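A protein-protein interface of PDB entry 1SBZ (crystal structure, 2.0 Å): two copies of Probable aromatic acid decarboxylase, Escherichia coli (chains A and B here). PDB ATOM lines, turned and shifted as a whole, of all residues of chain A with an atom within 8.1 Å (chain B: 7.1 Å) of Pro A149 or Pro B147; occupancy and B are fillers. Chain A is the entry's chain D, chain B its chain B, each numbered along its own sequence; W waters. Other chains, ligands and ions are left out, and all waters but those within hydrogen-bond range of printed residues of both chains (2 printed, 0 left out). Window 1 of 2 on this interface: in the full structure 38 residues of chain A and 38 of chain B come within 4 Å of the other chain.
O of Cys B86 sits at hydrogen-bond distance from N of Arg B122 (3.2 Å). N of Val B145 is in hydrogen-bond range of O of Leu B119. The guanidinium group (NH1) of Arg B122 lies within salt-bridge range of the side-chain carboxylate (OE1) of Glu B123 (3.8 Å). NH1 of Arg A122 lies within salt-bridge range of OE1 of Glu A123 (3.5 Å).
Pro B147 touches just these residues of chain A: Met A148 (3.7 Å) and Pro A149 (3.0 Å). Printed residues of chain B within 4 Å of Met A148: Pro B121 (3.5 Å), Arg B122 (2.8 Å), Glu B123 (3.5 Å), Pro B146 (3.8 Å) and Pro B147 (3.7 Å). Printed residues of chain B within 4 Å of Tyr A152: Thr B11 (3.3 Å). Of the printed residues of chain B, Met A124 touches Val B145, Pro B146 and Met B148. Pro B85 touches none of the printed residues of chain A. The nearest residue of chain A that does not touch Pro B147 is Pro A147 (4.2 Å).
Pro A146 touches Met B148, and with the chains exchanged Met A148 touches Pro B146. Pro A147 touches Met B148, and with the chains exchanged Met A148 touches Pro B147. Pro A147 touches Pro B149, and with the chains exchanged Pro A149 touches Pro B147. Ile B161 touches its own counterpart, Ile A161. Positions printed for both chains: 122, 123, 124, 146, 147, 148, 149, 150, 161, 162 and 165.
Water W1 bridges O of Pro A149 (2.7 Å) and O of Thr B11 (2.8 Å). Water W2 lies within hydrogen-bond range of the guanidinium group of Arg B122 (2.9 Å) and a ring nitrogen (NE2) of His A164 (3.1 Å).
The side-chain hydroxyl (OG1) of Thr B11 is in hydrogen-bond range of the backbone NH (N) of Phe A151. The side-chain hydroxyl of Thr B11 is in hydrogen-bond range of the backbone NH of Tyr A152, at 3.3 Å. The guanidinium group of Arg B122 lies within hydrogen-bond range of the backbone carbonyl oxygen of Met A148. NE of Arg B122 is in hydrogen-bond range of O of Pro A149 (2.9 Å). The backbone carbonyl oxygen (O) of Met B148 lies within hydrogen-bond range of the guanidinium group (NH2) of Arg A122 (3.0 Å). O of Pro B149 sits at hydrogen-bond distance from NE of Arg A122, at 3.0 Å. SD of Met A124 sits close to O of Pro B146 (3.2 Å). SD of Met B124 sits close to O of Pro A146. SD of Met A148 sits close to O of Pro B121, 3.5 Å away.
Among the printed residues, pairs that only touch across the chains: Pro A149 with Pro B147 (3.0 Å), Pro A147 with Pro B149 (3.0 Å), Phe A151 with Gly B12 (3.2 Å), Glu A123 with Met B148 (3.4 Å), Met A148 with Glu B123 (3.5 Å), Phe A151 with Val B158 (3.5 Å), Ile A161 with Ile B161 (3.6 Å), Ile A161 with Val B158 (3.7 Å), Pro A155 with Val B158 (3.7 Å), Met A148 with Pro B147 (3.7 Å), Phe A151 with Val B162 (3.7 Å), Pro A146 with Met B148 (3.8 Å), Met A148 with Pro B146 (3.8 Å), Ala A150 with Arg B122 (3.8 Å), Pro A147 with Met B148 (3.8 Å), Ala A150 with Thr B11 (3.8 Å), Arg A122 with Ala B150 (3.9 Å), Met A124 with Val B145 (3.9 Å), Met A124 with Met B148 (3.9 Å) and Pro A149 with Pro B149 (3.9 Å).
Of the 21 printed residues of chain B, 15 touch a printed residue of chain A. Along chain B the printed residues that touch a printed residue of chain A span positions 11 to 162. Printed residues of chain A that touch a printed residue of chain B: Arg A122, Glu A123, Met A124, Pro A146, Pro A147, Met A148, Pro A149, Ala A150, Phe A151, Tyr A152, Pro A155 and Ile A161. Hydrophobic or aromatic side chains of chain A that line the printed part of chain B: Met A124, Pro A146, Pro A147, Met A148, Pro A149, Ala A150, Phe A151, Tyr A152, Pro A155 and Ile A161. Among the printed residues, 29 pairs touch across the chains.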
ATOM      1  N   ARG A 122       1.524   4.258   5.102  1.00  0.00           N
ATOM      2  CA  ARG A 122       1.717   4.452   3.667  1.00  0.00           C
ATOM      3  C   ARG A 122       0.399   4.737   2.952  1.00  0.00           C
ATOM      4  O   ARG A 122      -0.518   3.912   2.937  1.00  0.00           O
ATOM      5  CB  ARG A 122       2.457   3.261   3.023  1.00  0.00           C
ATOM      6  CG  ARG A 122       3.006   3.525   1.617  1.00  0.00           C
ATOM      7  CD  ARG A 122       1.955   3.371   0.500  1.00  0.00           C
ATOM      8  NE  ARG A 122       2.345   4.047  -0.740  1.00  0.00           N
ATOM      9  CZ  ARG A 122       1.487   4.536  -1.627  1.00  0.00           C
ATOM     10  NH1 ARG A 122       0.176   4.437  -1.415  1.00  0.00           N
ATOM     11  NH2 ARG A 122       1.942   5.137  -2.726  1.00  0.00           N
ATOM     12  N   GLU A 123       0.337   5.935   2.375  1.00  0.00           N
ATOM     13  CA  GLU A 123      -0.775   6.410   1.569  1.00  0.00           C
ATOM     14  C   GLU A 123      -0.334   7.719   0.915  1.00  0.00           C
ATOM     15  O   GLU A 123       0.455   8.462   1.492  1.00  0.00           O
ATOM     16  CB  GLU A 123      -2.029   6.636   2.428  1.00  0.00           C
ATOM     17  CG  GLU A 123      -3.293   6.977   1.647  1.00  0.00           C
ATOM     18  CD  GLU A 123      -3.555   6.039   0.472  1.00  0.00           C
ATOM     19  OE1 GLU A 123      -2.826   6.108  -0.542  1.00  0.00           O
ATOM     20  OE2 GLU A 123      -4.510   5.252   0.550  1.00  0.00           O
ATOM     21  N   MET A 124      -0.826   7.985  -0.286  1.00  0.00           N
ATOM     22  CA  MET A 124      -0.540   9.234  -1.000  1.00  0.00           C
ATOM     23  C   MET A 124      -1.683   9.534  -1.977  1.00  0.00           C
ATOM     24  O   MET A 124      -2.119   8.631  -2.698  1.00  0.00           O
ATOM     25  CB  MET A 124       0.793   9.112  -1.740  1.00  0.00           C
ATOM     26  CG  MET A 124       1.049  10.141  -2.813  1.00  0.00           C
ATOM     27  SD  MET A 124       2.668   9.681  -3.805  1.00  0.00           S
ATOM     28  CE  MET A 124       1.852   8.264  -4.907  1.00  0.00           C
ATOM     29  N   PRO A 146       6.858   6.828   7.994  1.00  0.00           N
ATOM     30  CA  PRO A 146       6.413   6.584   6.629  1.00  0.00           C
ATOM     31  C   PRO A 146       7.625   6.234   5.771  1.00  0.00           C
ATOM     32  O   PRO A 146       8.717   6.734   6.054  1.00  0.00           O
ATOM     33  CB  PRO A 146       5.831   7.935   6.205  1.00  0.00           C
ATOM     34  CG  PRO A 146       6.578   8.928   7.018  1.00  0.00           C
ATOM     35  CD  PRO A 146       6.692   8.245   8.369  1.00  0.00           C
ATOM     36  N   PRO A 147       7.449   5.373   4.766  1.00  0.00           N
ATOM     37  CA  PRO A 147       8.554   4.924   3.927  1.00  0.00           C
ATOM     38  C   PRO A 147       9.008   5.953   2.886  1.00  0.00           C
ATOM     39  O   PRO A 147       8.919   5.695   1.695  1.00  0.00           O
ATOM     40  CB  PRO A 147       7.977   3.685   3.230  1.00  0.00           C
ATOM     41  CG  PRO A 147       6.505   3.926   3.172  1.00  0.00           C
ATOM     42  CD  PRO A 147       6.176   4.740   4.379  1.00  0.00           C
ATOM     43  N   MET A 148       9.529   7.085   3.339  1.00  0.00           N
ATOM     44  CA  MET A 148       9.994   8.158   2.459  1.00  0.00           C
ATOM     45  C   MET A 148      11.425   7.911   1.964  1.00  0.00           C
ATOM     46  O   MET A 148      12.339   7.827   2.778  1.00  0.00           O
ATOM     47  CB  MET A 148       9.985   9.480   3.229  1.00  0.00           C
ATOM     48  CG  MET A 148       8.692   9.773   3.957  1.00  0.00           C
ATOM     49  SD  MET A 148       7.790  11.213   3.073  1.00  0.00           S
ATOM     50  CE  MET A 148       6.580  11.815   4.571  1.00  0.00           C
ATOM     51  N   PRO A 149      11.620   7.815   0.645  1.00  0.00           N
ATOM     52  CA  PRO A 149      12.951   7.602   0.075  1.00  0.00           C
ATOM     53  C   PRO A 149      13.965   8.700   0.381  1.00  0.00           C
ATOM     54  O   PRO A 149      13.615   9.881   0.444  1.00  0.00           O
ATOM     55  CB  PRO A 149      12.684   7.513  -1.432  1.00  0.00           C
ATOM     56  CG  PRO A 149      11.391   8.149  -1.633  1.00  0.00           C
ATOM     57  CD  PRO A 149      10.583   7.851  -0.403  1.00  0.00           C
ATOM     58  N   ALA A 150      15.204   8.274   0.613  1.00  0.00           N
ATOM     59  CA  ALA A 150      16.346   9.160   0.772  1.00  0.00           C
ATOM     60  C   ALA A 150      17.183   9.060  -0.502  1.00  0.00           C
ATOM     61  O   ALA A 150      17.341   7.971  -1.059  1.00  0.00           O
ATOM     62  CB  ALA A 150      17.165   8.751   1.977  1.00  0.00           C
ATOM     63  N   PHE A 151      17.701  10.192  -0.969  1.00  0.00           N
ATOM     64  CA  PHE A 151      18.466  10.235  -2.220  1.00  0.00           C
ATOM     65  C   PHE A 151      19.926  10.666  -2.001  1.00  0.00           C
ATOM     66  O   PHE A 151      20.726  10.669  -2.937  1.00  0.00           O
ATOM     67  CB  PHE A 151      17.790  11.166  -3.239  1.00  0.00           C
ATOM     68  CG  PHE A 151      16.431  10.698  -3.683  1.00  0.00           C
ATOM     69  CD1 PHE A 151      15.299  10.979  -2.927  1.00  0.00           C
ATOM     70  CD2 PHE A 151      16.284   9.970  -4.856  1.00  0.00           C
ATOM     71  CE1 PHE A 151      14.031  10.543  -3.336  1.00  0.00           C
ATOM     72  CE2 PHE A 151      15.016   9.528  -5.266  1.00  0.00           C
ATOM     73  CZ  PHE A 151      13.894   9.815  -4.504  1.00  0.00           C
ATOM     74  N   TYR A 152      20.265  11.028  -0.770  1.00  0.00           N
ATOM     75  CA  TYR A 152      21.603  11.540  -0.469  1.00  0.00           C
ATOM     76  C   TYR A 152      22.684  10.460  -0.504  1.00  0.00           C
ATOM     77  O   TYR A 152      23.871  10.769  -0.669  1.00  0.00           O
ATOM     78  CB  TYR A 152      21.619  12.276   0.873  1.00  0.00           C
ATOM     79  CG  TYR A 152      21.292  11.421   2.080  1.00  0.00           C
ATOM     80  CD1 TYR A 152      20.020  11.451   2.655  1.00  0.00           C
ATOM     81  CD2 TYR A 152      22.259  10.602   2.663  1.00  0.00           C
ATOM     82  CE1 TYR A 152      19.716  10.675   3.773  1.00  0.00           C
ATOM     83  CE2 TYR A 152      21.963   9.825   3.778  1.00  0.00           C
ATOM     84  CZ  TYR A 152      20.690   9.867   4.321  1.00  0.00           C
ATOM     85  OH  TYR A 152      20.403   9.102   5.423  1.00  0.00           O
ATOM     86  N   ASN A 153      22.270   9.208  -0.317  1.00  0.00           N
ATOM     87  CA  ASN A 153      23.189   8.065  -0.313  1.00  0.00           C
ATOM     88  C   ASN A 153      23.233   7.378  -1.680  1.00  0.00           C
ATOM     89  O   ASN A 153      23.744   6.263  -1.813  1.00  0.00           O
ATOM     90  CB  ASN A 153      22.811   7.075   0.797  1.00  0.00           C
ATOM     91  CG  ASN A 153      21.320   6.764   0.824  1.00  0.00           C
ATOM     92  OD1 ASN A 153      20.597   7.031  -0.131  1.00  0.00           O
ATOM     93  ND2 ASN A 153      20.857   6.198   1.927  1.00  0.00           N
ATOM     94  N   PRO A 155      20.866   6.013  -4.022  1.00  0.00           N
ATOM     95  CA  PRO A 155      20.213   4.742  -4.318  1.00  0.00           C
ATOM     96  C   PRO A 155      20.074   4.519  -5.825  1.00  0.00           C
ATOM     97  O   PRO A 155      20.020   5.480  -6.606  1.00  0.00           O
ATOM     98  CB  PRO A 155      18.830   4.902  -3.679  1.00  0.00           C
ATOM     99  CG  PRO A 155      18.604   6.370  -3.656  1.00  0.00           C
ATOM    100  CD  PRO A 155      19.950   6.954  -3.348  1.00  0.00           C
ATOM    101  N   ASP A 160      17.531  -0.777  -2.644  1.00  0.00           N
ATOM    102  CA  ASP A 160      18.270   0.296  -1.966  1.00  0.00           C
ATOM    103  C   ASP A 160      17.358   1.123  -1.057  1.00  0.00           C
ATOM    104  O   ASP A 160      17.703   1.401   0.092  1.00  0.00           O
ATOM    105  CB  ASP A 160      18.935   1.240  -2.973  1.00  0.00           C
ATOM    106  CG  ASP A 160      20.194   0.659  -3.613  1.00  0.00           C
ATOM    107  OD1 ASP A 160      20.835  -0.226  -3.016  1.00  0.00           O
ATOM    108  OD2 ASP A 160      20.624   1.067  -4.718  1.00  0.00           O
ATOM    109  N   ILE A 161      16.201   1.509  -1.589  1.00  0.00           N
ATOM    110  CA  ILE A 161      15.230   2.315  -0.854  1.00  0.00           C
ATOM    111  C   ILE A 161      14.576   1.513   0.276  1.00  0.00           C
ATOM    112  O   ILE A 161      14.461   2.006   1.399  1.00  0.00           O
ATOM    113  CB  ILE A 161      14.185   2.923  -1.825  1.00  0.00           C
ATOM    114  CG1 ILE A 161      14.860   3.962  -2.728  1.00  0.00           C
ATOM    115  CG2 ILE A 161      13.008   3.552  -1.060  1.00  0.00           C
ATOM    116  CD1 ILE A 161      13.997   4.433  -3.872  1.00  0.00           C
ATOM    117  N   VAL A 162      14.171   0.279  -0.021  1.00  0.00           N
ATOM    118  CA  VAL A 162      13.550  -0.597   0.977  1.00  0.00           C
ATOM    119  C   VAL A 162      14.464  -0.792   2.192  1.00  0.00           C
ATOM    120  O   VAL A 162      14.024  -0.654   3.335  1.00  0.00           O
ATOM    121  CB  VAL A 162      13.150  -1.965   0.368  1.00  0.00           C
ATOM    122  CG1 VAL A 162      12.740  -2.960   1.455  1.00  0.00           C
ATOM    123  CG2 VAL A 162      12.022  -1.796  -0.641  1.00  0.00           C
ATOM    124  N   HIS A 164      16.995   1.005   3.260  1.00  0.00           N
ATOM    125  CA  HIS A 164      17.214   2.230   4.001  1.00  0.00           C
ATOM    126  C   HIS A 164      16.038   2.507   4.934  1.00  0.00           C
ATOM    127  O   HIS A 164      16.237   2.893   6.079  1.00  0.00           O
ATOM    128  CB  HIS A 164      17.439   3.407   3.056  1.00  0.00           C
ATOM    129  CG  HIS A 164      17.808   4.671   3.764  1.00  0.00           C
ATOM    130  ND1 HIS A 164      19.080   4.916   4.234  1.00  0.00           N
ATOM    131  CD2 HIS A 164      17.064   5.748   4.113  1.00  0.00           C
ATOM    132  CE1 HIS A 164      19.108   6.098   4.826  1.00  0.00           C
ATOM    133  NE2 HIS A 164      17.898   6.625   4.765  1.00  0.00           N
ATOM    134  N   VAL A 165      14.819   2.314   4.428  1.00  0.00           N
ATOM    135  CA  VAL A 165      13.608   2.487   5.228  1.00  0.00           C
ATOM    136  C   VAL A 165      13.642   1.522   6.405  1.00  0.00           C
ATOM    137  O   VAL A 165      13.460   1.931   7.548  1.00  0.00           O
ATOM    138  CB  VAL A 165      12.313   2.279   4.386  1.00  0.00           C
ATOM    139  CG1 VAL A 165      11.083   2.232   5.277  1.00  0.00           C
ATOM    140  CG2 VAL A 165      12.167   3.380   3.334  1.00  0.00           C
ATOM    141  N   THR B  11      15.939  15.910   1.235  1.00  0.00           N
ATOM    142  CA  THR B  11      16.462  14.893   0.334  1.00  0.00           C
ATOM    143  C   THR B  11      15.340  14.481  -0.618  1.00  0.00           C
ATOM    144  O   THR B  11      14.201  14.319  -0.197  1.00  0.00           O
ATOM    145  CB  THR B  11      17.089  13.711   1.117  1.00  0.00           C
ATOM    146  OG1 THR B  11      17.712  12.799   0.206  1.00  0.00           O
ATOM    147  CG2 THR B  11      16.037  12.862   1.828  1.00  0.00           C
ATOM    148  N   GLY B  12      15.656  14.366  -1.906  1.00  0.00           N
ATOM    149  CA  GLY B  12      14.642  14.130  -2.932  1.00  0.00           C
ATOM    150  C   GLY B  12      14.670  15.168  -4.042  1.00  0.00           C
ATOM    151  O   GLY B  12      13.663  15.405  -4.710  1.00  0.00           O
ATOM    152  N   LEU B  15      13.263  14.388  -7.393  1.00  0.00           N
ATOM    153  CA  LEU B  15      11.811  14.533  -7.519  1.00  0.00           C
ATOM    154  C   LEU B  15      11.458  15.839  -8.234  1.00  0.00           C
ATOM    155  O   LEU B  15      10.640  15.847  -9.155  1.00  0.00           O
ATOM    156  CB  LEU B  15      11.120  14.471  -6.141  1.00  0.00           C
ATOM    157  CG  LEU B  15      11.148  13.145  -5.361  1.00  0.00           C
ATOM    158  CD1 LEU B  15      10.741  13.368  -3.923  1.00  0.00           C
ATOM    159  CD2 LEU B  15      10.259  12.072  -5.997  1.00  0.00           C
ATOM    160  N   PRO B  85      11.064  18.750  -3.405  1.00  0.00           N
ATOM    161  CA  PRO B  85      10.369  18.236  -2.217  1.00  0.00           C
ATOM    162  C   PRO B  85      10.225  19.389  -1.237  1.00  0.00           C
ATOM    163  O   PRO B  85      10.869  20.425  -1.417  1.00  0.00           O
ATOM    164  CB  PRO B  85      11.354  17.208  -1.658  1.00  0.00           C
ATOM    165  CG  PRO B  85      12.711  17.775  -2.042  1.00  0.00           C
ATOM    166  CD  PRO B  85      12.493  18.394  -3.411  1.00  0.00           C
ATOM    167  N   CYS B  86       9.379  19.220  -0.232  1.00  0.00           N
ATOM    168  CA  CYS B  86       9.155  20.264   0.767  1.00  0.00           C
ATOM    169  C   CYS B  86       9.743  19.836   2.104  1.00  0.00           C
ATOM    170  O   CYS B  86       9.270  18.873   2.699  1.00  0.00           O
ATOM    171  CB  CYS B  86       7.654  20.533   0.917  1.00  0.00           C
ATOM    172  SG  CYS B  86       7.252  21.890   2.049  1.00  0.00           S
ATOM    173  N   LEU B 119       2.014  20.418  -1.771  1.00  0.00           N
ATOM    174  CA  LEU B 119       3.284  20.200  -1.099  1.00  0.00           C
ATOM    175  C   LEU B 119       3.707  18.747  -1.201  1.00  0.00           C
ATOM    176  O   LEU B 119       2.878  17.854  -1.085  1.00  0.00           O
ATOM    177  CB  LEU B 119       3.132  20.566   0.372  1.00  0.00           C
ATOM    178  CG  LEU B 119       3.552  21.917   0.936  1.00  0.00           C
ATOM    179  CD1 LEU B 119       3.561  23.069  -0.062  1.00  0.00           C
ATOM    180  CD2 LEU B 119       2.726  22.229   2.172  1.00  0.00           C
ATOM    181  N   VAL B 120       5.002  18.525  -1.399  1.00  0.00           N
ATOM    182  CA  VAL B 120       5.593  17.184  -1.424  1.00  0.00           C
ATOM    183  C   VAL B 120       6.495  17.054  -0.185  1.00  0.00           C
ATOM    184  O   VAL B 120       7.721  17.138  -0.289  1.00  0.00           O
ATOM    185  CB  VAL B 120       6.352  16.927  -2.784  1.00  0.00           C
ATOM    186  CG1 VAL B 120       6.918  15.502  -2.877  1.00  0.00           C
ATOM    187  CG2 VAL B 120       5.424  17.195  -3.963  1.00  0.00           C
ATOM    188  N   PRO B 121       5.886  16.886   0.996  1.00  0.00           N
ATOM    189  CA  PRO B 121       6.645  16.849   2.237  1.00  0.00           C
ATOM    190  C   PRO B 121       7.472  15.584   2.324  1.00  0.00           C
ATOM    191  O   PRO B 121       6.976  14.491   2.034  1.00  0.00           O
ATOM    192  CB  PRO B 121       5.554  16.840   3.314  1.00  0.00           C
ATOM    193  CG  PRO B 121       4.398  16.203   2.638  1.00  0.00           C
ATOM    194  CD  PRO B 121       4.441  16.694   1.240  1.00  0.00           C
ATOM    195  N   ARG B 122       8.732  15.737   2.712  1.00  0.00           N
ATOM    196  CA  ARG B 122       9.616  14.592   2.851  1.00  0.00           C
ATOM    197  C   ARG B 122      10.432  14.728   4.124  1.00  0.00           C
ATOM    198  O   ARG B 122      11.200  15.682   4.280  1.00  0.00           O
ATOM    199  CB  ARG B 122      10.532  14.438   1.629  1.00  0.00           C
ATOM    200  CG  ARG B 122      11.260  13.102   1.566  1.00  0.00           C
ATOM    201  CD  ARG B 122      12.526  13.012   2.436  1.00  0.00           C
ATOM    202  NE  ARG B 122      12.940  11.625   2.654  1.00  0.00           N
ATOM    203  CZ  ARG B 122      13.588  11.184   3.729  1.00  0.00           C
ATOM    204  NH1 ARG B 122      13.934  12.013   4.704  1.00  0.00           N
ATOM    205  NH2 ARG B 122      13.900   9.899   3.824  1.00  0.00           N
ATOM    206  N   GLU B 123      10.227  13.767   5.019  1.00  0.00           N
ATOM    207  CA  GLU B 123      10.940  13.635   6.289  1.00  0.00           C
ATOM    208  C   GLU B 123      10.525  12.309   6.901  1.00  0.00           C
ATOM    209  O   GLU B 123       9.413  11.838   6.671  1.00  0.00           O
ATOM    210  CB  GLU B 123      10.608  14.785   7.251  1.00  0.00           C
ATOM    211  CG  GLU B 123      11.380  14.790   8.572  1.00  0.00           C
ATOM    212  CD  GLU B 123      12.890  14.698   8.390  1.00  0.00           C
ATOM    213  OE1 GLU B 123      13.383  13.586   8.111  1.00  0.00           O
ATOM    214  OE2 GLU B 123      13.588  15.729   8.528  1.00  0.00           O
ATOM    215  N   MET B 124      11.407  11.711   7.690  1.00  0.00           N
ATOM    216  CA  MET B 124      11.134  10.413   8.286  1.00  0.00           C
ATOM    217  C   MET B 124      12.083  10.210   9.485  1.00  0.00           C
ATOM    218  O   MET B 124      13.286  10.424   9.337  1.00  0.00           O
ATOM    219  CB  MET B 124      11.352   9.356   7.196  1.00  0.00           C
ATOM    220  CG  MET B 124      10.773   8.000   7.424  1.00  0.00           C
ATOM    221  SD  MET B 124      12.138   6.727   6.780  1.00  0.00           S
ATOM    222  CE  MET B 124      13.422   7.484   7.902  1.00  0.00           C
ATOM    223  N   VAL B 145       1.249  15.581  -0.655  1.00  0.00           N
ATOM    224  CA  VAL B 145       1.614  14.512  -1.571  1.00  0.00           C
ATOM    225  C   VAL B 145       3.040  14.045  -1.272  1.00  0.00           C
ATOM    226  O   VAL B 145       3.963  14.310  -2.046  1.00  0.00           O
ATOM    227  CB  VAL B 145       1.436  14.954  -3.056  1.00  0.00           C
ATOM    228  CG1 VAL B 145       1.627  13.785  -4.007  1.00  0.00           C
ATOM    229  CG2 VAL B 145       0.057  15.558  -3.272  1.00  0.00           C
ATOM    230  N   PRO B 146       3.217  13.331  -0.156  1.00  0.00           N
ATOM    231  CA  PRO B 146       4.535  12.841   0.227  1.00  0.00           C
ATOM    232  C   PRO B 146       5.010  11.804  -0.805  1.00  0.00           C
ATOM    233  O   PRO B 146       4.170  11.147  -1.406  1.00  0.00           O
ATOM    234  CB  PRO B 146       4.290  12.198   1.598  1.00  0.00           C
ATOM    235  CG  PRO B 146       2.858  11.839   1.609  1.00  0.00           C
ATOM    236  CD  PRO B 146       2.170  12.873   0.772  1.00  0.00           C
ATOM    237  N   PRO B 147       6.319  11.681  -1.043  1.00  0.00           N
ATOM    238  CA  PRO B 147       6.826  10.694  -2.007  1.00  0.00           C
ATOM    239  C   PRO B 147       6.779   9.272  -1.452  1.00  0.00           C
ATOM    240  O   PRO B 147       7.807   8.720  -1.073  1.00  0.00           O
ATOM    241  CB  PRO B 147       8.277  11.134  -2.234  1.00  0.00           C
ATOM    242  CG  PRO B 147       8.667  11.825  -0.981  1.00  0.00           C
ATOM    243  CD  PRO B 147       7.407  12.461  -0.430  1.00  0.00           C
ATOM    244  N   MET B 148       5.588   8.692  -1.385  1.00  0.00           N
ATOM    245  CA  MET B 148       5.420   7.350  -0.850  1.00  0.00           C
ATOM    246  C   MET B 148       5.507   6.339  -1.989  1.00  0.00           C
ATOM    247  O   MET B 148       4.657   6.357  -2.875  1.00  0.00           O
ATOM    248  CB  MET B 148       4.049   7.211  -0.186  1.00  0.00           C
ATOM    249  CG  MET B 148       3.759   8.218   0.894  1.00  0.00           C
ATOM    250  SD  MET B 148       4.255   7.562   2.646  1.00  0.00           S
ATOM    251  CE  MET B 148       3.188   8.842   3.704  1.00  0.00           C
ATOM    252  N   PRO B 149       6.510   5.458  -1.964  1.00  0.00           N
ATOM    253  CA  PRO B 149       6.657   4.432  -3.002  1.00  0.00           C
ATOM    254  C   PRO B 149       5.437   3.515  -3.118  1.00  0.00           C
ATOM    255  O   PRO B 149       4.846   3.104  -2.110  1.00  0.00           O
ATOM    256  CB  PRO B 149       7.886   3.633  -2.551  1.00  0.00           C
ATOM    257  CG  PRO B 149       8.631   4.543  -1.644  1.00  0.00           C
ATOM    258  CD  PRO B 149       7.583   5.381  -0.957  1.00  0.00           C
ATOM    259  N   ALA B 150       5.057   3.237  -4.360  1.00  0.00           N
ATOM    260  CA  ALA B 150       4.014   2.276  -4.660  1.00  0.00           C
ATOM    261  C   ALA B 150       4.678   1.027  -5.224  1.00  0.00           C
ATOM    262  O   ALA B 150       5.540   1.118  -6.109  1.00  0.00           O
ATOM    263  CB  ALA B 150       3.031   2.863  -5.654  1.00  0.00           C
ATOM    264  N   VAL B 158      15.006   3.344  -8.947  1.00  0.00           N
ATOM    265  CA  VAL B 158      14.658   4.611  -8.301  1.00  0.00           C
ATOM    266  C   VAL B 158      13.883   5.528  -9.264  1.00  0.00           C
ATOM    267  O   VAL B 158      12.959   6.221  -8.842  1.00  0.00           O
ATOM    268  CB  VAL B 158      15.924   5.305  -7.726  1.00  0.00           C
ATOM    269  CG1 VAL B 158      15.646   6.745  -7.299  1.00  0.00           C
ATOM    270  CG2 VAL B 158      16.479   4.507  -6.558  1.00  0.00           C
ATOM    271  N   ILE B 161      10.042   4.795  -9.176  1.00  0.00           N
ATOM    272  CA  ILE B 161       9.394   5.417  -8.018  1.00  0.00           C
ATOM    273  C   ILE B 161       9.255   6.924  -8.206  1.00  0.00           C
ATOM    274  O   ILE B 161       8.190   7.484  -7.963  1.00  0.00           O
ATOM    275  CB  ILE B 161      10.166   5.089  -6.717  1.00  0.00           C
ATOM    276  CG1 ILE B 161      10.053   3.596  -6.405  1.00  0.00           C
ATOM    277  CG2 ILE B 161       9.626   5.920  -5.540  1.00  0.00           C
ATOM    278  CD1 ILE B 161      11.075   3.101  -5.416  1.00  0.00           C
ATOM    279  N   VAL B 162      10.331   7.565  -8.659  1.00  0.00           N
ATOM    280  CA  VAL B 162      10.329   8.999  -8.942  1.00  0.00           C
ATOM    281  C   VAL B 162       9.267   9.366  -9.985  1.00  0.00           C
ATOM    282  O   VAL B 162       8.500  10.320  -9.797  1.00  0.00           O
ATOM    283  CB  VAL B 162      11.728   9.489  -9.378  1.00  0.00           C
ATOM    284  CG1 VAL B 162      11.665  10.884  -9.998  1.00  0.00           C
ATOM    285  CG2 VAL B 162      12.684   9.470  -8.199  1.00  0.00           C
ATOM    286  N   VAL B 165       5.659   9.221  -8.419  1.00  0.00           N
ATOM    287  CA  VAL B 165       5.374  10.378  -7.564  1.00  0.00           C
ATOM    288  C   VAL B 165       5.086  11.633  -8.397  1.00  0.00           C
ATOM    289  O   VAL B 165       4.117  12.346  -8.132  1.00  0.00           O
ATOM    290  CB  VAL B 165       6.540  10.642  -6.577  1.00  0.00           C
ATOM    291  CG1 VAL B 165       6.351  11.965  -5.821  1.00  0.00           C
ATOM    292  CG2 VAL B 165       6.673   9.483  -5.605  1.00  0.00           C
HETATM  293  O   HOH W   1      12.749  12.088  -0.930  1.00  0.00           O
HETATM  294  O   HOH W   2      15.546   8.397   5.610  1.00  0.00           O
